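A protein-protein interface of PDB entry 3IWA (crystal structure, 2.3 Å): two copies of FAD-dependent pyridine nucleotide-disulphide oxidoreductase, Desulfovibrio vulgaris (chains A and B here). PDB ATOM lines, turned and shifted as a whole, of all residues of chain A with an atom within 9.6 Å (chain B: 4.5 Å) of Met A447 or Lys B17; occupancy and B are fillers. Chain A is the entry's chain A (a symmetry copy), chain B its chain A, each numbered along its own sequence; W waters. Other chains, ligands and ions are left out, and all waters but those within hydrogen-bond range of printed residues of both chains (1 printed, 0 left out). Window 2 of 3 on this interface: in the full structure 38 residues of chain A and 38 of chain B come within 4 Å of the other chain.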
ATOM      1  N   VAL A 371      18.420  15.797  10.208  1.00  0.00           N
ATOM      2  CA  VAL A 371      17.103  15.364  10.529  1.00  0.00           C
ATOM      3  C   VAL A 371      17.219  13.914  10.911  1.00  0.00           C
ATOM      4  O   VAL A 371      17.968  13.177  10.273  1.00  0.00           O
ATOM      5  CB  VAL A 371      16.214  15.463   9.294  1.00  0.00           C
ATOM      6  CG1 VAL A 371      15.018  14.621   9.488  1.00  0.00           C
ATOM      7  CG2 VAL A 371      15.846  16.931   9.006  1.00  0.00           C
ATOM      8  N   GLU A 372      16.509  13.512  11.967  1.00  0.00           N
ATOM      9  CA  GLU A 372      16.457  12.100  12.407  1.00  0.00           C
ATOM     10  C   GLU A 372      15.017  11.619  12.465  1.00  0.00           C
ATOM     11  O   GLU A 372      14.105  12.434  12.573  1.00  0.00           O
ATOM     12  CB  GLU A 372      17.107  11.905  13.786  1.00  0.00           C
ATOM     13  CG  GLU A 372      18.589  12.250  13.827  1.00  0.00           C
ATOM     14  CD  GLU A 372      18.842  13.745  13.770  1.00  0.00           C
ATOM     15  OE1 GLU A 372      18.071  14.503  14.400  1.00  0.00           O
ATOM     16  OE2 GLU A 372      19.813  14.168  13.113  1.00  0.00           O
ATOM     17  N   GLN A 373      14.820  10.300  12.397  1.00  0.00           N
ATOM     18  CA  GLN A 373      13.475   9.691  12.410  1.00  0.00           C
ATOM     19  C   GLN A 373      13.409   8.507  13.378  1.00  0.00           C
ATOM     20  O   GLN A 373      14.261   7.611  13.340  1.00  0.00           O
ATOM     21  CB  GLN A 373      13.084   9.246  11.002  1.00  0.00           C
ATOM     22  CG  GLN A 373      11.678   8.622  10.866  1.00  0.00           C
ATOM     23  CD  GLN A 373      11.342   8.256   9.414  1.00  0.00           C
ATOM     24  OE1 GLN A 373      11.497   7.104   8.997  1.00  0.00           O
ATOM     25  NE2 GLN A 373      10.901   9.242   8.636  1.00  0.00           N
ATOM     26  N   LEU A 388      19.455  11.899   8.059  1.00  0.00           N
ATOM     27  CA  LEU A 388      19.860  12.598   6.858  1.00  0.00           C
ATOM     28  C   LEU A 388      20.526  13.907   7.221  1.00  0.00           C
ATOM     29  O   LEU A 388      20.075  14.605   8.130  1.00  0.00           O
ATOM     30  CB  LEU A 388      18.657  12.967   5.990  1.00  0.00           C
ATOM     31  CG  LEU A 388      17.862  11.868   5.325  1.00  0.00           C
ATOM     32  CD1 LEU A 388      16.850  12.522   4.358  1.00  0.00           C
ATOM     33  CD2 LEU A 388      18.814  10.862   4.622  1.00  0.00           C
ATOM     34  N   ARG A 415      16.125   7.448  -0.311  1.00  0.00           N
ATOM     35  CA  ARG A 415      16.083   8.830   0.063  1.00  0.00           C
ATOM     36  C   ARG A 415      17.274   9.509  -0.610  1.00  0.00           C
ATOM     37  O   ARG A 415      17.152  10.557  -1.200  1.00  0.00           O
ATOM     38  CB  ARG A 415      16.162   8.919   1.599  1.00  0.00           C
ATOM     39  CG  ARG A 415      14.914   9.339   2.390  1.00  0.00           C
ATOM     40  CD  ARG A 415      13.569   8.727   2.048  1.00  0.00           C
ATOM     41  NE  ARG A 415      13.522   7.351   2.462  1.00  0.00           N
ATOM     42  CZ  ARG A 415      12.444   6.695   2.867  1.00  0.00           C
ATOM     43  NH1 ARG A 415      12.588   5.420   3.194  1.00  0.00           N
ATOM     44  NH2 ARG A 415      11.244   7.272   2.959  1.00  0.00           N
ATOM     45  N   ILE A 432      13.650  20.564  -2.622  1.00  0.00           N
ATOM     46  CA  ILE A 432      13.719  19.440  -1.693  1.00  0.00           C
ATOM     47  C   ILE A 432      12.455  19.389  -0.808  1.00  0.00           C
ATOM     48  O   ILE A 432      11.881  18.333  -0.619  1.00  0.00           O
ATOM     49  CB  ILE A 432      14.964  19.483  -0.811  1.00  0.00           C
ATOM     50  CG1 ILE A 432      16.239  19.568  -1.641  1.00  0.00           C
ATOM     51  CG2 ILE A 432      15.004  18.273   0.116  1.00  0.00           C
ATOM     52  CD1 ILE A 432      16.365  18.608  -2.782  1.00  0.00           C
ATOM     53  N   SER A 433      11.983  20.539  -0.337  1.00  0.00           N
ATOM     54  CA  SER A 433      10.654  20.639   0.324  1.00  0.00           C
ATOM     55  C   SER A 433       9.535  20.030  -0.551  1.00  0.00           C
ATOM     56  O   SER A 433       8.629  19.405  -0.062  1.00  0.00           O
ATOM     57  CB  SER A 433      10.274  22.117   0.668  1.00  0.00           C
ATOM     58  OG  SER A 433      11.146  22.707   1.624  1.00  0.00           O
ATOM     59  N   ASN A 434       9.597  20.278  -1.837  1.00  0.00           N
ATOM     60  CA  ASN A 434       8.574  19.816  -2.774  1.00  0.00           C
ATOM     61  C   ASN A 434       8.897  18.522  -3.535  1.00  0.00           C
ATOM     62  O   ASN A 434       8.085  18.112  -4.352  1.00  0.00           O
ATOM     63  CB  ASN A 434       8.267  20.927  -3.783  1.00  0.00           C
ATOM     64  CG  ASN A 434       7.519  22.072  -3.161  1.00  0.00           C
ATOM     65  OD1 ASN A 434       6.900  21.916  -2.136  1.00  0.00           O
ATOM     66  ND2 ASN A 434       7.568  23.236  -3.794  1.00  0.00           N
ATOM     67  N   ALA A 435      10.043  17.886  -3.268  1.00  0.00           N
ATOM     68  CA  ALA A 435      10.492  16.709  -4.030  1.00  0.00           C
ATOM     69  C   ALA A 435       9.386  15.696  -4.049  1.00  0.00           C
ATOM     70  O   ALA A 435       8.860  15.351  -3.007  1.00  0.00           O
ATOM     71  CB  ALA A 435      11.745  16.078  -3.417  1.00  0.00           C
ATOM     72  N   VAL A 437       8.602  12.611  -3.935  1.00  0.00           N
ATOM     73  CA  VAL A 437       8.999  11.286  -3.557  1.00  0.00           C
ATOM     74  C   VAL A 437       7.768  10.489  -3.260  1.00  0.00           C
ATOM     75  O   VAL A 437       6.755  11.003  -2.806  1.00  0.00           O
ATOM     76  CB  VAL A 437       9.970  11.246  -2.359  1.00  0.00           C
ATOM     77  CG1 VAL A 437      11.248  12.049  -2.686  1.00  0.00           C
ATOM     78  CG2 VAL A 437       9.310  11.752  -1.081  1.00  0.00           C
ATOM     79  N   VAL A 438       7.879   9.220  -3.579  1.00  0.00           N
ATOM     80  CA  VAL A 438       6.820   8.264  -3.418  1.00  0.00           C
ATOM     81  C   VAL A 438       6.501   8.128  -1.937  1.00  0.00           C
ATOM     82  O   VAL A 438       7.401   7.788  -1.173  1.00  0.00           O
ATOM     83  CB  VAL A 438       7.301   6.885  -3.988  1.00  0.00           C
ATOM     84  CG1 VAL A 438       6.590   5.772  -3.321  1.00  0.00           C
ATOM     85  CG2 VAL A 438       7.133   6.844  -5.507  1.00  0.00           C
ATOM     86  N   MET A 447       4.876  13.548   6.731  1.00  0.00           N
ATOM     87  CA  MET A 447       5.631  13.663   5.466  1.00  0.00           C
ATOM     88  C   MET A 447       6.991  12.954   5.461  1.00  0.00           C
ATOM     89  O   MET A 447       7.537  12.582   6.506  1.00  0.00           O
ATOM     90  CB  MET A 447       5.768  15.121   4.981  1.00  0.00           C
ATOM     91  CG  MET A 447       6.270  16.129   5.986  1.00  0.00           C
ATOM     92  SD  MET A 447       5.537  17.774   5.750  1.00  0.00           S
ATOM     93  CE  MET A 447       5.953  18.159   4.042  1.00  0.00           C
ATOM     94  N   ASP A 448       7.490  12.731   4.249  1.00  0.00           N
ATOM     95  CA  ASP A 448       8.717  12.003   4.018  1.00  0.00           C
ATOM     96  C   ASP A 448       9.922  12.793   4.561  1.00  0.00           C
ATOM     97  O   ASP A 448       9.937  14.021   4.530  1.00  0.00           O
ATOM     98  CB  ASP A 448       8.871  11.748   2.521  1.00  0.00           C
ATOM     99  CG  ASP A 448       9.948  10.713   2.203  1.00  0.00           C
ATOM    100  OD1 ASP A 448      11.141  11.074   2.145  1.00  0.00           O
ATOM    101  OD2 ASP A 448       9.580   9.543   1.994  1.00  0.00           O
ATOM    102  N   ILE A 449      10.914  12.069   5.058  1.00  0.00           N
ATOM    103  CA  ILE A 449      12.072  12.676   5.670  1.00  0.00           C
ATOM    104  C   ILE A 449      12.850  13.575   4.739  1.00  0.00           C
ATOM    105  O   ILE A 449      13.394  14.567   5.179  1.00  0.00           O
ATOM    106  CB  ILE A 449      12.972  11.626   6.378  1.00  0.00           C
ATOM    107  CG1 ILE A 449      14.028  12.357   7.228  1.00  0.00           C
ATOM    108  CG2 ILE A 449      13.565  10.649   5.390  1.00  0.00           C
ATOM    109  CD1 ILE A 449      14.965  11.458   7.987  1.00  0.00           C
ATOM    110  N   VAL A 450      12.837  13.295   3.441  1.00  0.00           N
ATOM    111  CA  VAL A 450      13.509  14.157   2.482  1.00  0.00           C
ATOM    112  C   VAL A 450      12.868  15.546   2.430  1.00  0.00           C
ATOM    113  O   VAL A 450      13.573  16.553   2.384  1.00  0.00           O
ATOM    114  CB  VAL A 450      13.498  13.556   1.059  1.00  0.00           C
ATOM    115  CG1 VAL A 450      13.805  14.626   0.028  1.00  0.00           C
ATOM    116  CG2 VAL A 450      14.512  12.434   0.962  1.00  0.00           C
ATOM    117  N   ASN A 451      11.537  15.583   2.381  1.00  0.00           N
ATOM    118  CA  ASN A 451      10.797  16.839   2.420  1.00  0.00           C
ATOM    119  C   ASN A 451      11.049  17.542   3.763  1.00  0.00           C
ATOM    120  O   ASN A 451      11.231  18.738   3.823  1.00  0.00           O
ATOM    121  CB  ASN A 451       9.273  16.609   2.258  1.00  0.00           C
ATOM    122  CG  ASN A 451       8.868  16.024   0.894  1.00  0.00           C
ATOM    123  OD1 ASN A 451       7.998  15.171   0.839  1.00  0.00           O
ATOM    124  ND2 ASN A 451       9.474  16.499  -0.194  1.00  0.00           N
ATOM    125  N   VAL A 452      11.048  16.780   4.846  1.00  0.00           N
ATOM    126  CA  VAL A 452      11.277  17.359   6.170  1.00  0.00           C
ATOM    127  C   VAL A 452      12.664  18.016   6.190  1.00  0.00           C
ATOM    128  O   VAL A 452      12.799  19.107   6.684  1.00  0.00           O
ATOM    129  CB  VAL A 452      11.084  16.306   7.282  1.00  0.00           C
ATOM    130  CG1 VAL A 452      11.527  16.849   8.703  1.00  0.00           C
ATOM    131  CG2 VAL A 452       9.607  15.810   7.283  1.00  0.00           C
ATOM    132  N   ALA A 453      13.668  17.407   5.570  1.00  0.00           N
ATOM    133  CA  ALA A 453      15.002  18.011   5.548  1.00  0.00           C
ATOM    134  C   ALA A 453      14.965  19.349   4.831  1.00  0.00           C
ATOM    135  O   ALA A 453      15.618  20.290   5.259  1.00  0.00           O
ATOM    136  CB  ALA A 453      16.033  17.078   4.899  1.00  0.00           C
ATOM    137  N   GLY A 454      14.233  19.426   3.722  1.00  0.00           N
ATOM    138  CA  GLY A 454      14.074  20.693   2.996  1.00  0.00           C
ATOM    139  C   GLY A 454      13.348  21.776   3.810  1.00  0.00           C
ATOM    140  O   GLY A 454      13.683  22.943   3.731  1.00  0.00           O
ATOM    141  N   ASN A 455      12.374  21.375   4.615  1.00  0.00           N
ATOM    142  CA  ASN A 455      11.644  22.323   5.472  1.00  0.00           C
ATOM    143  C   ASN A 455      12.523  22.853   6.626  1.00  0.00           C
ATOM    144  O   ASN A 455      12.559  24.065   6.865  1.00  0.00           O
ATOM    145  CB  ASN A 455      10.364  21.677   6.019  1.00  0.00           C
ATOM    146  CG  ASN A 455       9.349  21.302   4.897  1.00  0.00           C
ATOM    147  OD1 ASN A 455       9.463  21.697   3.725  1.00  0.00           O
ATOM    148  ND2 ASN A 455       8.370  20.546   5.281  1.00  0.00           N
ATOM    149  N   VAL A 456      13.240  21.952   7.302  1.00  0.00           N
ATOM    150  CA  VAL A 456      14.201  22.351   8.326  1.00  0.00           C
ATOM    151  C   VAL A 456      15.297  23.268   7.781  1.00  0.00           C
ATOM    152  O   VAL A 456      15.633  24.265   8.407  1.00  0.00           O
ATOM    153  CB  VAL A 456      14.840  21.162   9.039  1.00  0.00           C
ATOM    154  CG1 VAL A 456      15.905  21.663  10.008  1.00  0.00           C
ATOM    155  CG2 VAL A 456      13.791  20.330   9.750  1.00  0.00           C
ATOM    156  N   ASN A 459      13.810  26.640   7.156  1.00  0.00           N
ATOM    157  CA  ASN A 459      13.743  27.210   8.500  1.00  0.00           C
ATOM    158  C   ASN A 459      15.118  27.674   9.065  1.00  0.00           C
ATOM    159  O   ASN A 459      15.249  28.805   9.581  1.00  0.00           O
ATOM    160  CB  ASN A 459      13.077  26.215   9.471  1.00  0.00           C
ATOM    161  CG  ASN A 459      11.589  26.046   9.208  1.00  0.00           C
ATOM    162  OD1 ASN A 459      10.990  26.795   8.439  1.00  0.00           O
ATOM    163  ND2 ASN A 459      11.002  25.037   9.815  1.00  0.00           N
ATOM    164  N   ALA B  13      -5.934  17.428   5.331  1.00  0.00           N
ATOM    165  CA  ALA B  13      -4.603  17.654   5.818  1.00  0.00           C
ATOM    166  C   ALA B  13      -4.342  19.121   5.513  1.00  0.00           C
ATOM    167  O   ALA B  13      -3.853  19.847   6.357  1.00  0.00           O
ATOM    168  CB  ALA B  13      -3.604  16.743   5.086  1.00  0.00           C
ATOM    169  N   LEU B  14      -4.743  19.554   4.323  1.00  0.00           N
ATOM    170  CA  LEU B  14      -4.301  20.818   3.814  1.00  0.00           C
ATOM    171  C   LEU B  14      -4.617  22.051   4.682  1.00  0.00           C
ATOM    172  O   LEU B  14      -3.736  22.893   4.870  1.00  0.00           O
ATOM    173  CB  LEU B  14      -4.751  21.017   2.369  1.00  0.00           C
ATOM    174  CG  LEU B  14      -4.123  22.259   1.732  1.00  0.00           C
ATOM    175  CD1 LEU B  14      -3.305  21.926   0.492  1.00  0.00           C
ATOM    176  CD2 LEU B  14      -5.211  23.287   1.411  1.00  0.00           C
ATOM    177  N   GLY B  15      -5.845  22.155   5.190  1.00  0.00           N
ATOM    178  CA  GLY B  15      -6.262  23.290   6.027  1.00  0.00           C
ATOM    179  C   GLY B  15      -5.401  23.483   7.263  1.00  0.00           C
ATOM    180  O   GLY B  15      -4.740  24.512   7.395  1.00  0.00           O
ATOM    181  N   PRO B  16      -5.374  22.479   8.164  1.00  0.00           N
ATOM    182  CA  PRO B  16      -4.501  22.492   9.354  1.00  0.00           C
ATOM    183  C   PRO B  16      -3.037  22.792   9.018  1.00  0.00           C
ATOM    184  O   PRO B  16      -2.383  23.567   9.721  1.00  0.00           O
ATOM    185  CB  PRO B  16      -4.641  21.073   9.921  1.00  0.00           C
ATOM    186  CG  PRO B  16      -5.985  20.619   9.455  1.00  0.00           C
ATOM    187  CD  PRO B  16      -6.203  21.265   8.107  1.00  0.00           C
ATOM    188  N   LYS B  17      -2.528  22.211   7.936  1.00  0.00           N
ATOM    189  CA  LYS B  17      -1.134  22.475   7.544  1.00  0.00           C
ATOM    190  C   LYS B  17      -0.935  23.938   7.195  1.00  0.00           C
ATOM    191  O   LYS B  17       0.000  24.559   7.644  1.00  0.00           O
ATOM    192  CB  LYS B  17      -0.720  21.608   6.351  1.00  0.00           C
ATOM    193  CG  LYS B  17       0.778  21.655   6.025  1.00  0.00           C
ATOM    194  CD  LYS B  17       1.604  21.066   7.181  1.00  0.00           C
ATOM    195  CE  LYS B  17       3.121  21.014   6.887  1.00  0.00           C
ATOM    196  NZ  LYS B  17       3.844  20.051   7.839  1.00  0.00           N
ATOM    197  N   ALA B  18      -1.804  24.477   6.367  1.00  0.00           N
ATOM    198  CA  ALA B  18      -1.658  25.852   5.938  1.00  0.00           C
ATOM    199  C   ALA B  18      -1.701  26.814   7.151  1.00  0.00           C
ATOM    200  O   ALA B  18      -0.906  27.738   7.244  1.00  0.00           O
ATOM    201  CB  ALA B  18      -2.703  26.202   4.911  1.00  0.00           C
ATOM    202  N   ALA B  19      -2.598  26.538   8.084  1.00  0.00           N
ATOM    203  CA  ALA B  19      -2.853  27.410   9.199  1.00  0.00           C
ATOM    204  C   ALA B  19      -1.689  27.347  10.183  1.00  0.00           C
ATOM    205  O   ALA B  19      -1.224  28.377  10.649  1.00  0.00           O
ATOM    206  CB  ALA B  19      -4.156  27.014   9.875  1.00  0.00           C
ATOM    207  N   CYS B  20      -1.238  26.136  10.506  1.00  0.00           N
ATOM    208  CA  CYS B  20      -0.101  25.951  11.398  1.00  0.00           C
ATOM    209  C   CYS B  20       1.182  26.588  10.856  1.00  0.00           C
ATOM    210  O   CYS B  20       1.942  27.220  11.596  1.00  0.00           O
ATOM    211  CB  CYS B  20       0.144  24.473  11.644  1.00  0.00           C
ATOM    212  SG  CYS B  20       1.650  24.202  12.543  1.00  0.00           S
ATOM    213  N   ARG B  21       1.428  26.442   9.564  1.00  0.00           N
ATOM    214  CA  ARG B  21       2.585  27.100   8.953  1.00  0.00           C
ATOM    215  C   ARG B  21       2.408  28.629   8.988  1.00  0.00           C
ATOM    216  O   ARG B  21       3.357  29.389   9.247  1.00  0.00           O
ATOM    217  CB  ARG B  21       2.746  26.624   7.509  1.00  0.00           C
ATOM    218  CG  ARG B  21       3.700  27.404   6.668  1.00  0.00           C
ATOM    219  CD  ARG B  21       5.149  27.288   7.134  1.00  0.00           C
ATOM    220  NE  ARG B  21       6.047  27.978   6.198  1.00  0.00           N
ATOM    221  CZ  ARG B  21       7.342  28.173   6.416  1.00  0.00           C
ATOM    222  NH1 ARG B  21       7.911  27.709   7.512  1.00  0.00           N
ATOM    223  NH2 ARG B  21       8.075  28.807   5.525  1.00  0.00           N
ATOM    224  N   ASN B 316       0.275  18.129   2.297  1.00  0.00           N
ATOM    225  CA  ASN B 316       1.298  18.718   3.129  1.00  0.00           C
ATOM    226  C   ASN B 316       2.204  19.683   2.390  1.00  0.00           C
ATOM    227  O   ASN B 316       2.474  20.754   2.896  1.00  0.00           O
ATOM    228  CB  ASN B 316       2.077  17.655   3.914  1.00  0.00           C
ATOM    229  CG  ASN B 316       1.271  17.159   5.115  1.00  0.00           C
ATOM    230  OD1 ASN B 316       0.369  17.875   5.573  1.00  0.00           O
ATOM    231  ND2 ASN B 316       1.567  15.944   5.623  1.00  0.00           N
ATOM    232  N   GLY B 319       0.131  22.779   1.323  1.00  0.00           N
ATOM    233  CA  GLY B 319      -0.291  23.492   2.511  1.00  0.00           C
ATOM    234  C   GLY B 319       0.794  24.395   3.037  1.00  0.00           C
ATOM    235  O   GLY B 319       0.525  25.545   3.428  1.00  0.00           O
ATOM    236  N   ARG B 320       2.026  23.879   3.036  1.00  0.00           N
ATOM    237  CA  ARG B 320       3.158  24.637   3.509  1.00  0.00           C
ATOM    238  C   ARG B 320       3.321  25.873   2.678  1.00  0.00           C
ATOM    239  O   ARG B 320       3.484  26.947   3.211  1.00  0.00           O
ATOM    240  CB  ARG B 320       4.423  23.815   3.483  1.00  0.00           C
ATOM    241  CG  ARG B 320       5.579  24.522   4.126  1.00  0.00           C
ATOM    242  CD  ARG B 320       6.775  23.574   4.280  1.00  0.00           C
ATOM    243  NE  ARG B 320       7.679  24.019   5.332  1.00  0.00           N
ATOM    244  CZ  ARG B 320       8.716  24.814   5.159  1.00  0.00           C
ATOM    245  NH1 ARG B 320       9.446  25.126   6.206  1.00  0.00           N
ATOM    246  NH2 ARG B 320       9.036  25.295   3.968  1.00  0.00           N
HETATM  247  O   HOH W   1       8.406  23.881   8.368  1.00  0.00           O
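NZ of Lys B17 is in hydrogen-bond range of SD of Met A447 (3.5 Å). NH1 of Arg B21 is in hydrogen-bond range of OD1 of Asn A459 (3.3 Å). The guanidinium group (NE) of Arg B320 lies close to the side-chain amide oxygen (OD1) of Asn A455 (3.3 Å). The side-chain amide oxygen of Asn A459 is in hydrogen-bond range of the guanidinium group of Arg B320, 3.2 Å away.
OD1 of Asn A455 is in hydrogen-bond range of OG of Ser A433 (2.9 Å). OD1 of Asn A455 sits close to O of Asn A451 (3.4 Å). The backbone carbonyl oxygen (O) of Asn A455 lies close to the side-chain amide nitrogen (ND2) of Asn A459 (3.5 Å).
Among the printed residues, pairs that only touch across the chains: Met A447 with Asn B316 (3.9 Å).
Met A447 touches two residues of chain B. Of chain A, only Met A447 (3.5 Å) comes within 4 Å of Lys B17. No residue of chain A comes within 4 Å of Gly B15. No residue of chain A comes within 4 Å of Ala B19. Asn B316 touches just one residue of chain A: Met A447. No residue of chain A comes within 4 Å of Gly B319. Printed residues of chain A within 4 Å of Arg B320: Asn A455 and Asn A459. Printed residues of chain B within 4 Å of Asn A459: Arg B21 (3.3 Å) and Arg B320 (3.2 Å). Leu A388 touches none of the printed residues of chain B. The nearest printed residue of chain B that does not touch Met A447 is Arg B320 (5.5 Å).
Of the 12 printed residues of chain B, 4 touch a printed residue of chain A. Of the 22 printed residues of chain A, 3 touch a printed residue of chain B. Hydrophobic or aromatic side chains of chain A that line the printed part of chain B: Met A447.
No position is printed for both chains.
Water W1 bridges the guanidinium group of Arg B320 (2.7 Å) and the side-chain amide nitrogen of Asn A459 (3.2 Å).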
